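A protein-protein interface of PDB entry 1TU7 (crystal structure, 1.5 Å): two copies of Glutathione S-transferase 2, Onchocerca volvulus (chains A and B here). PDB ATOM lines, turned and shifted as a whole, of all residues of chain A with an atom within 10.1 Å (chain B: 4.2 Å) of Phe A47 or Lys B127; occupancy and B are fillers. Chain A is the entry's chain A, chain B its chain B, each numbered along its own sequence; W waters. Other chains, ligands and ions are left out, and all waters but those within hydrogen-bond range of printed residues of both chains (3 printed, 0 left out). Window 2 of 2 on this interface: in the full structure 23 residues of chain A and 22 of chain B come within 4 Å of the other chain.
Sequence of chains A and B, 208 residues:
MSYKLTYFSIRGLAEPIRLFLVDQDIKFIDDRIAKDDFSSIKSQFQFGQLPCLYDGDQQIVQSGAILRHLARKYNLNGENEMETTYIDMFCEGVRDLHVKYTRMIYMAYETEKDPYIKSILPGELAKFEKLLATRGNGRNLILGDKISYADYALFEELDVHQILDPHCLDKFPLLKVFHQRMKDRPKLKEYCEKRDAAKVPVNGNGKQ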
ATOM      1  N   PHE A  38      -5.572 -23.144  35.135  1.00  0.00           N
ATOM      2  CA  PHE A  38      -4.512 -23.134  34.137  1.00  0.00           C
ATOM      3  C   PHE A  38      -3.573 -21.936  34.255  1.00  0.00           C
ATOM      4  O   PHE A  38      -2.353 -22.087  34.104  1.00  0.00           O
ATOM      5  CB  PHE A  38      -5.072 -23.220  32.714  1.00  0.00           C
ATOM      6  CG  PHE A  38      -3.999 -23.353  31.684  1.00  0.00           C
ATOM      7  CD1 PHE A  38      -3.081 -24.380  31.786  1.00  0.00           C
ATOM      8  CD2 PHE A  38      -3.874 -22.443  30.640  1.00  0.00           C
ATOM      9  CE1 PHE A  38      -2.033 -24.498  30.882  1.00  0.00           C
ATOM     10  CE2 PHE A  38      -2.830 -22.564  29.715  1.00  0.00           C
ATOM     11  CZ  PHE A  38      -1.926 -23.592  29.838  1.00  0.00           C
ATOM     12  N   ILE A  41      -0.295 -22.243  36.164  1.00  0.00           N
ATOM     13  CA  ILE A  41       0.700 -23.196  35.679  1.00  0.00           C
ATOM     14  C   ILE A  41       1.127 -22.934  34.231  1.00  0.00           C
ATOM     15  O   ILE A  41       2.041 -23.585  33.765  1.00  0.00           O
ATOM     16  CB  ILE A  41       0.201 -24.677  35.811  1.00  0.00           C
ATOM     17  CG1 ILE A  41      -1.111 -24.937  35.090  1.00  0.00           C
ATOM     18  CG2 ILE A  41       0.061 -25.103  37.293  1.00  0.00           C
ATOM     19  CD1 ILE A  41      -1.410 -26.467  34.927  1.00  0.00           C
ATOM     20  N   LYS A  42       0.480 -21.985  33.558  1.00  0.00           N
ATOM     21  CA  LYS A  42       0.644 -21.762  32.109  1.00  0.00           C
ATOM     22  C   LYS A  42       2.103 -21.587  31.672  1.00  0.00           C
ATOM     23  O   LYS A  42       2.514 -22.084  30.628  1.00  0.00           O
ATOM     24  CB  LYS A  42      -0.196 -20.560  31.690  1.00  0.00           C
ATOM     25  CG  LYS A  42      -0.101 -20.152  30.266  1.00  0.00           C
ATOM     26  CD  LYS A  42      -0.773 -18.792  30.048  1.00  0.00           C
ATOM     27  CE  LYS A  42      -0.718 -18.383  28.566  1.00  0.00           C
ATOM     28  NZ  LYS A  42      -1.529 -19.228  27.586  1.00  0.00           N
ATOM     29  N   SER A  43       2.887 -20.884  32.468  1.00  0.00           N
ATOM     30  CA  SER A  43       4.281 -20.612  32.119  1.00  0.00           C
ATOM     31  C   SER A  43       5.168 -21.858  32.123  1.00  0.00           C
ATOM     32  O   SER A  43       6.262 -21.841  31.564  1.00  0.00           O
ATOM     33  CB  SER A  43       4.884 -19.543  33.046  1.00  0.00           C
ATOM     34  OG  SER A  43       5.064 -20.053  34.332  1.00  0.00           O
ATOM     35  N   GLN A  44       4.689 -22.945  32.729  1.00  0.00           N
ATOM     36  CA  GLN A  44       5.427 -24.201  32.731  1.00  0.00           C
ATOM     37  C   GLN A  44       5.460 -24.906  31.375  1.00  0.00           C
ATOM     38  O   GLN A  44       6.242 -25.825  31.206  1.00  0.00           O
ATOM     39  CB  GLN A  44       4.799 -25.155  33.722  1.00  0.00           C
ATOM     40  CG  GLN A  44       4.824 -24.612  35.150  1.00  0.00           C
ATOM     41  CD  GLN A  44       4.265 -25.582  36.142  1.00  0.00           C
ATOM     42  OE1 GLN A  44       4.110 -26.767  35.849  1.00  0.00           O
ATOM     43  NE2 GLN A  44       3.972 -25.092  37.341  1.00  0.00           N
ATOM     44  N   PHE A  45       4.612 -24.479  30.453  1.00  0.00           N
ATOM     45  CA  PHE A  45       4.459 -25.104  29.128  1.00  0.00           C
ATOM     46  C   PHE A  45       5.122 -24.234  28.096  1.00  0.00           C
ATOM     47  O   PHE A  45       4.990 -23.028  28.148  1.00  0.00           O
ATOM     48  CB  PHE A  45       2.981 -25.347  28.864  1.00  0.00           C
ATOM     49  CG  PHE A  45       2.380 -26.186  29.939  1.00  0.00           C
ATOM     50  CD1 PHE A  45       1.695 -25.596  30.983  1.00  0.00           C
ATOM     51  CD2 PHE A  45       2.640 -27.542  30.004  1.00  0.00           C
ATOM     52  CE1 PHE A  45       1.207 -26.359  32.045  1.00  0.00           C
ATOM     53  CE2 PHE A  45       2.149 -28.313  31.041  1.00  0.00           C
ATOM     54  CZ  PHE A  45       1.434 -27.728  32.064  1.00  0.00           C
ATOM     55  N   GLN A  46       5.823 -24.863  27.160  1.00  0.00           N
ATOM     56  CA  GLN A  46       6.705 -24.155  26.247  1.00  0.00           C
ATOM     57  C   GLN A  46       6.013 -23.103  25.366  1.00  0.00           C
ATOM     58  O   GLN A  46       6.628 -22.106  25.014  1.00  0.00           O
ATOM     59  CB  GLN A  46       7.484 -25.163  25.396  1.00  0.00           C
ATOM     60  CG  GLN A  46       8.469 -26.016  26.193  1.00  0.00           C
ATOM     61  CD  GLN A  46       7.965 -27.415  26.574  1.00  0.00           C
ATOM     62  OE1 GLN A  46       8.723 -28.418  26.507  1.00  0.00           O
ATOM     63  NE2 GLN A  46       6.730 -27.487  27.004  1.00  0.00           N
ATOM     64  N   PHE A  47       4.750 -23.315  25.000  1.00  0.00           N
ATOM     65  CA  PHE A  47       3.951 -22.312  24.314  1.00  0.00           C
ATOM     66  C   PHE A  47       2.772 -21.791  25.132  1.00  0.00           C
ATOM     67  O   PHE A  47       1.877 -21.183  24.594  1.00  0.00           O
ATOM     68  CB  PHE A  47       3.498 -22.822  22.934  1.00  0.00           C
ATOM     69  CG  PHE A  47       4.645 -23.176  22.051  1.00  0.00           C
ATOM     70  CD1 PHE A  47       5.002 -24.495  21.786  1.00  0.00           C
ATOM     71  CD2 PHE A  47       5.418 -22.160  21.527  1.00  0.00           C
ATOM     72  CE1 PHE A  47       6.098 -24.759  20.987  1.00  0.00           C
ATOM     73  CE2 PHE A  47       6.440 -22.381  20.744  1.00  0.00           C
ATOM     74  CZ  PHE A  47       6.842 -23.698  20.512  1.00  0.00           C
ATOM     75  N   GLY A  48       2.785 -22.064  26.432  1.00  0.00           N
ATOM     76  CA  GLY A  48       1.725 -21.623  27.316  1.00  0.00           C
ATOM     77  C   GLY A  48       0.403 -22.309  27.093  1.00  0.00           C
ATOM     78  O   GLY A  48      -0.647 -21.784  27.458  1.00  0.00           O
ATOM     79  N   GLN A  49       0.443 -23.493  26.473  1.00  0.00           N
ATOM     80  CA  GLN A  49      -0.766 -24.204  26.060  1.00  0.00           C
ATOM     81  C   GLN A  49      -0.649 -25.716  26.315  1.00  0.00           C
ATOM     82  O   GLN A  49       0.415 -26.266  26.588  1.00  0.00           O
ATOM     83  CB  GLN A  49      -1.049 -23.912  24.573  1.00  0.00           C
ATOM     84  CG  GLN A  49      -1.437 -22.445  24.341  1.00  0.00           C
ATOM     85  CD  GLN A  49      -2.217 -22.217  23.075  1.00  0.00           C
ATOM     86  OE1 GLN A  49      -3.317 -21.617  23.100  1.00  0.00           O
ATOM     87  NE2 GLN A  49      -1.694 -22.683  21.981  1.00  0.00           N
ATOM     88  N   LEU A  50      -1.803 -26.358  26.261  1.00  0.00           N
ATOM     89  CA  LEU A  50      -1.959 -27.801  26.427  1.00  0.00           C
ATOM     90  C   LEU A  50      -2.509 -28.361  25.112  1.00  0.00           C
ATOM     91  O   LEU A  50      -3.113 -27.627  24.339  1.00  0.00           O
ATOM     92  CB  LEU A  50      -2.932 -28.067  27.580  1.00  0.00           C
ATOM     93  CG  LEU A  50      -2.501 -27.483  28.935  1.00  0.00           C
ATOM     94  CD1 LEU A  50      -3.531 -27.796  30.027  1.00  0.00           C
ATOM     95  CD2 LEU A  50      -1.132 -27.943  29.343  1.00  0.00           C
ATOM     96  N   PRO A  51      -2.372 -29.656  24.825  1.00  0.00           N
ATOM     97  CA  PRO A  51      -1.906 -30.701  25.731  1.00  0.00           C
ATOM     98  C   PRO A  51      -0.419 -30.757  25.930  1.00  0.00           C
ATOM     99  O   PRO A  51       0.347 -30.220  25.120  1.00  0.00           O
ATOM    100  CB  PRO A  51      -2.385 -31.977  25.029  1.00  0.00           C
ATOM    101  CG  PRO A  51      -2.380 -31.632  23.598  1.00  0.00           C
ATOM    102  CD  PRO A  51      -2.850 -30.217  23.552  1.00  0.00           C
ATOM    103  N   CYS A  52      -0.036 -31.361  27.046  1.00  0.00           N
ATOM    104  CA  CYS A  52       1.352 -31.711  27.348  1.00  0.00           C
ATOM    105  C   CYS A  52       1.471 -33.142  27.737  1.00  0.00           C
ATOM    106  O   CYS A  52       0.723 -33.583  28.597  1.00  0.00           O
ATOM    107  CB  CYS A  52       1.832 -30.833  28.491  1.00  0.00           C
ATOM    108  SG  CYS A  52       3.540 -31.076  28.978  1.00  0.00           S
ATOM    109  N   GLN A  59       9.235 -33.379  28.733  1.00  0.00           N
ATOM    110  CA  GLN A  59       8.036 -32.608  28.671  1.00  0.00           C
ATOM    111  C   GLN A  59       7.801 -32.184  27.224  1.00  0.00           C
ATOM    112  O   GLN A  59       8.559 -31.388  26.647  1.00  0.00           O
ATOM    113  CB  GLN A  59       8.129 -31.377  29.580  1.00  0.00           C
ATOM    114  CG  GLN A  59       6.853 -30.565  29.585  1.00  0.00           C
ATOM    115  CD  GLN A  59       6.952 -29.167  30.172  1.00  0.00           C
ATOM    116  OE1 GLN A  59       8.023 -28.576  30.189  1.00  0.00           O
ATOM    117  NE2 GLN A  59       5.820 -28.603  30.555  1.00  0.00           N
ATOM    118  N   ILE A  60       6.722 -32.726  26.633  1.00  0.00           N
ATOM    119  CA  ILE A  60       6.420 -32.536  25.225  1.00  0.00           C
ATOM    120  C   ILE A  60       5.063 -31.863  25.069  1.00  0.00           C
ATOM    121  O   ILE A  60       4.034 -32.435  25.437  1.00  0.00           O
ATOM    122  CB  ILE A  60       6.404 -33.888  24.501  1.00  0.00           C
ATOM    123  CG1 ILE A  60       7.656 -34.688  24.825  1.00  0.00           C
ATOM    124  CG2 ILE A  60       6.278 -33.642  23.003  1.00  0.00           C
ATOM    125  CD1 ILE A  60       7.544 -36.137  24.428  1.00  0.00           C
ATOM    126  N   VAL A  61       5.037 -30.648  24.547  1.00  0.00           N
ATOM    127  CA  VAL A  61       3.807 -30.025  24.118  1.00  0.00           C
ATOM    128  C   VAL A  61       3.676 -30.158  22.589  1.00  0.00           C
ATOM    129  O   VAL A  61       4.564 -30.722  21.941  1.00  0.00           O
ATOM    130  CB  VAL A  61       3.672 -28.552  24.608  1.00  0.00           C
ATOM    131  CG1 VAL A  61       3.616 -28.507  26.114  1.00  0.00           C
ATOM    132  CG2 VAL A  61       4.790 -27.648  24.082  1.00  0.00           C
ATOM    133  N   GLN A  62       2.534 -29.691  22.069  1.00  0.00           N
ATOM    134  CA  GLN A  62       2.119 -29.770  20.670  1.00  0.00           C
ATOM    135  C   GLN A  62       1.550 -31.141  20.374  1.00  0.00           C
ATOM    136  O   GLN A  62       2.267 -32.120  20.260  1.00  0.00           O
ATOM    137  CB  GLN A  62       3.219 -29.368  19.685  1.00  0.00           C
ATOM    138  CG  GLN A  62       3.542 -27.884  19.744  1.00  0.00           C
ATOM    139  CD  GLN A  62       2.493 -26.968  19.165  1.00  0.00           C
ATOM    140  OE1 GLN A  62       2.570 -25.722  19.335  1.00  0.00           O
ATOM    141  NE2 GLN A  62       1.547 -27.522  18.486  1.00  0.00           N
ATOM    142  N   SER A  63       0.232 -31.182  20.205  1.00  0.00           N
ATOM    143  CA  SER A  63      -0.472 -32.429  20.043  1.00  0.00           C
ATOM    144  C   SER A  63       0.101 -33.285  18.927  1.00  0.00           C
ATOM    145  O   SER A  63       0.200 -34.489  19.088  1.00  0.00           O
ATOM    146  CB  SER A  63      -1.961 -32.201  19.817  1.00  0.00           C
ATOM    147  OG  SER A  63      -2.232 -31.473  18.622  1.00  0.00           O
ATOM    148  N   ALA A  65       3.211 -33.310  17.742  1.00  0.00           N
ATOM    149  CA  ALA A  65       4.532 -33.793  18.153  1.00  0.00           C
ATOM    150  C   ALA A  65       4.410 -34.905  19.191  1.00  0.00           C
ATOM    151  O   ALA A  65       5.160 -35.858  19.170  1.00  0.00           O
ATOM    152  CB  ALA A  65       5.391 -32.661  18.710  1.00  0.00           C
ATOM    153  N   ILE A  66       3.426 -34.779  20.077  1.00  0.00           N
ATOM    154  CA  ILE A  66       3.159 -35.806  21.077  1.00  0.00           C
ATOM    155  C   ILE A  66       2.774 -37.095  20.377  1.00  0.00           C
ATOM    156  O   ILE A  66       3.317 -38.168  20.664  1.00  0.00           O
ATOM    157  CB  ILE A  66       2.041 -35.352  22.057  1.00  0.00           C
ATOM    158  CG1 ILE A  66       2.488 -34.169  22.923  1.00  0.00           C
ATOM    159  CG2 ILE A  66       1.596 -36.539  22.922  1.00  0.00           C
ATOM    160  CD1 ILE A  66       1.358 -33.447  23.642  1.00  0.00           C
ATOM    161  N   MET B  89       8.013 -30.308  17.949  1.00  0.00           N
ATOM    162  CA  MET B  89       7.351 -29.406  18.881  1.00  0.00           C
ATOM    163  C   MET B  89       7.594 -27.925  18.502  1.00  0.00           C
ATOM    164  O   MET B  89       6.686 -27.115  18.401  1.00  0.00           O
ATOM    165  CB  MET B  89       7.810 -29.729  20.306  1.00  0.00           C
ATOM    166  CG  MET B  89       7.260 -28.826  21.314  1.00  0.00           C
ATOM    167  SD  MET B  89       7.961 -29.244  22.946  1.00  0.00           S
ATOM    168  CE  MET B  89       9.488 -28.382  22.890  1.00  0.00           C
ATOM    169  N   GLY B  93       5.040 -25.132  16.923  1.00  0.00           N
ATOM    170  CA  GLY B  93       4.816 -23.828  17.514  1.00  0.00           C
ATOM    171  C   GLY B  93       4.944 -22.709  16.485  1.00  0.00           C
ATOM    172  O   GLY B  93       4.191 -21.737  16.524  1.00  0.00           O
ATOM    173  N   GLY B 123       4.497 -11.457  23.051  1.00  0.00           N
ATOM    174  CA  GLY B 123       4.384 -12.611  23.936  1.00  0.00           C
ATOM    175  C   GLY B 123       4.665 -13.908  23.192  1.00  0.00           C
ATOM    176  O   GLY B 123       5.184 -14.865  23.767  1.00  0.00           O
ATOM    177  N   GLU B 124       4.287 -13.970  21.918  1.00  0.00           N
ATOM    178  CA  GLU B 124       4.556 -15.161  21.131  1.00  0.00           C
ATOM    179  C   GLU B 124       6.020 -15.298  20.806  1.00  0.00           C
ATOM    180  O   GLU B 124       6.558 -16.404  20.875  1.00  0.00           O
ATOM    181  CB  GLU B 124       3.697 -15.214  19.880  1.00  0.00           C
ATOM    182  CG  GLU B 124       2.222 -15.263  20.224  1.00  0.00           C
ATOM    183  CD  GLU B 124       1.922 -16.376  21.220  1.00  0.00           C
ATOM    184  OE1 GLU B 124       1.523 -16.098  22.393  1.00  0.00           O
ATOM    185  OE2 GLU B 124       2.160 -17.543  20.902  1.00  0.00           O
ATOM    186  N   LEU B 125       6.660 -14.199  20.442  1.00  0.00           N
ATOM    187  CA  LEU B 125       8.112 -14.230  20.248  1.00  0.00           C
ATOM    188  C   LEU B 125       8.860 -14.595  21.521  1.00  0.00           C
ATOM    189  O   LEU B 125       9.846 -15.326  21.460  1.00  0.00           O
ATOM    190  CB  LEU B 125       8.595 -12.897  19.635  1.00  0.00           C
ATOM    191  CG  LEU B 125       8.096 -12.591  18.217  1.00  0.00           C
ATOM    192  CD1 LEU B 125       8.568 -11.182  17.828  1.00  0.00           C
ATOM    193  CD2 LEU B 125       8.513 -13.620  17.159  1.00  0.00           C
ATOM    194  N   ALA B 126       8.391 -14.119  22.672  1.00  0.00           N
ATOM    195  CA  ALA B 126       9.061 -14.394  23.916  1.00  0.00           C
ATOM    196  C   ALA B 126       9.085 -15.889  24.171  1.00  0.00           C
ATOM    197  O   ALA B 126      10.045 -16.405  24.702  1.00  0.00           O
ATOM    198  CB  ALA B 126       8.391 -13.681  25.053  1.00  0.00           C
ATOM    199  N   LYS B 127       8.052 -16.614  23.742  1.00  0.00           N
ATOM    200  CA  LYS B 127       8.041 -18.047  23.950  1.00  0.00           C
ATOM    201  C   LYS B 127       9.164 -18.679  23.145  1.00  0.00           C
ATOM    202  O   LYS B 127       9.866 -19.569  23.650  1.00  0.00           O
ATOM    203  CB  LYS B 127       6.677 -18.662  23.586  1.00  0.00           C
ATOM    204  CG  LYS B 127       5.579 -18.257  24.547  1.00  0.00           C
ATOM    205  CD  LYS B 127       4.185 -18.471  23.973  1.00  0.00           C
ATOM    206  CE  LYS B 127       3.135 -18.162  25.004  1.00  0.00           C
ATOM    207  NZ  LYS B 127       1.742 -18.155  24.455  1.00  0.00           N
ATOM    208  N   PHE B 128       9.349 -18.236  21.901  1.00  0.00           N
ATOM    209  CA  PHE B 128      10.417 -18.766  21.079  1.00  0.00           C
ATOM    210  C   PHE B 128      11.806 -18.366  21.596  1.00  0.00           C
ATOM    211  O   PHE B 128      12.736 -19.168  21.529  1.00  0.00           O
ATOM    212  CB  PHE B 128      10.272 -18.312  19.631  1.00  0.00           C
ATOM    213  CG  PHE B 128       9.117 -18.963  18.908  1.00  0.00           C
ATOM    214  CD1 PHE B 128       8.016 -18.225  18.543  1.00  0.00           C
ATOM    215  CD2 PHE B 128       9.183 -20.304  18.586  1.00  0.00           C
ATOM    216  CE1 PHE B 128       6.972 -18.837  17.849  1.00  0.00           C
ATOM    217  CE2 PHE B 128       8.142 -20.913  17.925  1.00  0.00           C
ATOM    218  CZ  PHE B 128       7.048 -20.170  17.570  1.00  0.00           C
ATOM    219  N   GLU B 129      11.951 -17.138  22.067  1.00  0.00           N
ATOM    220  CA  GLU B 129      13.230 -16.672  22.596  1.00  0.00           C
ATOM    221  C   GLU B 129      13.660 -17.550  23.770  1.00  0.00           C
ATOM    222  O   GLU B 129      14.815 -17.939  23.893  1.00  0.00           O
ATOM    223  CB  GLU B 129      13.070 -15.216  23.030  1.00  0.00           C
ATOM    224  CG  GLU B 129      14.332 -14.554  23.572  1.00  0.00           C
ATOM    225  CD  GLU B 129      15.353 -14.142  22.535  1.00  0.00           C
ATOM    226  OE1 GLU B 129      15.078 -14.207  21.338  1.00  0.00           O
ATOM    227  OE2 GLU B 129      16.487 -13.760  22.967  1.00  0.00           O
ATOM    228  N   LYS B 130      12.712 -17.882  24.630  1.00  0.00           N
ATOM    229  CA  LYS B 130      12.982 -18.738  25.761  1.00  0.00           C
ATOM    230  C   LYS B 130      13.331 -20.160  25.327  1.00  0.00           C
ATOM    231  O   LYS B 130      14.236 -20.777  25.863  1.00  0.00           O
ATOM    232  CB  LYS B 130      11.788 -18.733  26.729  1.00  0.00           C
ATOM    233  CG  LYS B 130      12.062 -19.515  27.984  1.00  0.00           C
ATOM    234  CD  LYS B 130      11.018 -19.286  29.044  1.00  0.00           C
ATOM    235  CE  LYS B 130      11.284 -20.209  30.232  1.00  0.00           C
ATOM    236  NZ  LYS B 130      10.452 -19.799  31.382  1.00  0.00           N
ATOM    237  N   LEU B 131      12.564 -20.695  24.376  1.00  0.00           N
ATOM    238  CA  LEU B 131      12.720 -22.087  23.990  1.00  0.00           C
ATOM    239  C   LEU B 131      14.035 -22.255  23.244  1.00  0.00           C
ATOM    240  O   LEU B 131      14.758 -23.216  23.437  1.00  0.00           O
ATOM    241  CB  LEU B 131      11.516 -22.535  23.160  1.00  0.00           C
ATOM    242  CG  LEU B 131      11.423 -24.011  22.821  1.00  0.00           C
ATOM    243  CD1 LEU B 131      11.360 -24.859  24.068  1.00  0.00           C
ATOM    244  CD2 LEU B 131      10.181 -24.204  21.967  1.00  0.00           C
HETATM  245  O   HOH W   1       0.617 -19.424  22.087  1.00  0.00           O
HETATM  246  O   HOH W   2       7.785 -19.808  30.513  1.00  0.00           O
HETATM  247  O   HOH W   3       8.787 -20.851  25.902  1.00  0.00           O
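Of the 11 printed residues of chain B, 5 touch a printed residue of chain A. Hydrophobic or aromatic side chains of chain B that line the printed part of chain A: Met B89, Phe B128 and Leu B131. Hydrophobic or aromatic side chains of chain A that line the printed part of chain B: Phe A47, Val A61 and Ala A65. Along chain A the printed residues that touch a printed residue of chain B span positions 46 to 65. Among the printed residues, no Asp or Glu carboxylate lies within 4 Å of a Lys or Arg side-chain nitrogen of the other chain.
OE1 of Gln A46 lies close to O of Gln A59, 3.0 Å away. The side-chain amino group (NZ) of Lys B127 lies within salt-bridge range of the side-chain carboxylate (OE1) of Glu B124, 2.9 Å away.
Water W3 bridges the backbone carbonyl oxygen of Gln A46 (2.7 Å) and the backbone carbonyl oxygen of Lys B127 (2.8 Å). Water W1 lies within hydrogen-bond range of the side-chain carboxylate of Glu B124 (2.7 Å), the side-chain amino group of Lys B127 (2.9 Å) and the backbone carbonyl oxygen of Phe A47 (3.3 Å). Water W2 bridges O of Ser A43 (2.7 Å) and NZ of Lys B130 (2.8 Å).
Of the printed residues of chain B, Gln A46 touches Met B89 (3.7 Å), Lys B127 (3.7 Å) and Leu B131 (3.8 Å). Of chain B, only Met B89, Gly B93, Lys B127, Phe B128 and Leu B131 come within 4 Å of Phe A47. Leu A50 touches none of the printed residues of chain B. Ile A66 touches none of the printed residues of chain B. Printed residues of chain A within 4 Å of Met B89: Gln A46 (3.7 Å), Phe A47 (3.5 Å), Val A61 (3.4 Å), Gln A62 (3.5 Å) and Ala A65 (3.6 Å). No residue of chain A comes within 4 Å of Glu B124. Lys B127 touches just these residues of chain A: Gln A46 and Phe A47. Printed residues of chain A within 4 Å of Leu B131: Gln A46 (3.8 Å) and Phe A47 (3.7 Å).
Gln A46 touches Lys B127 (O to CB, 3.7 Å). Leu B131 touches Gln A46. Phe A47 touches Met B89. CZ of Phe A47 touches CA of Gly B93, 3.6 Å away. CE2 of Phe B128 touches CE2 of Phe A47, at 3.6 Å. Phe A47 touches Leu B131. O of Met B89 touches CG of Gln A62, 3.5 Å away. Gly B93 touches Gln A62 (CA to OE1, 3.5 Å). Ala A65 touches Met B89.
OE1 of Gln A46 sits close to SD of Met B89. The backbone carbonyl oxygen (O) of Phe A47 sits at hydrogen-bond distance from the side-chain amino group (NZ) of Lys B127 (3.0 Å). N of Val A61 lies within hydrogen-bond range of SD of Met B89 (3.6 Å).
No position is printed for both chains.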
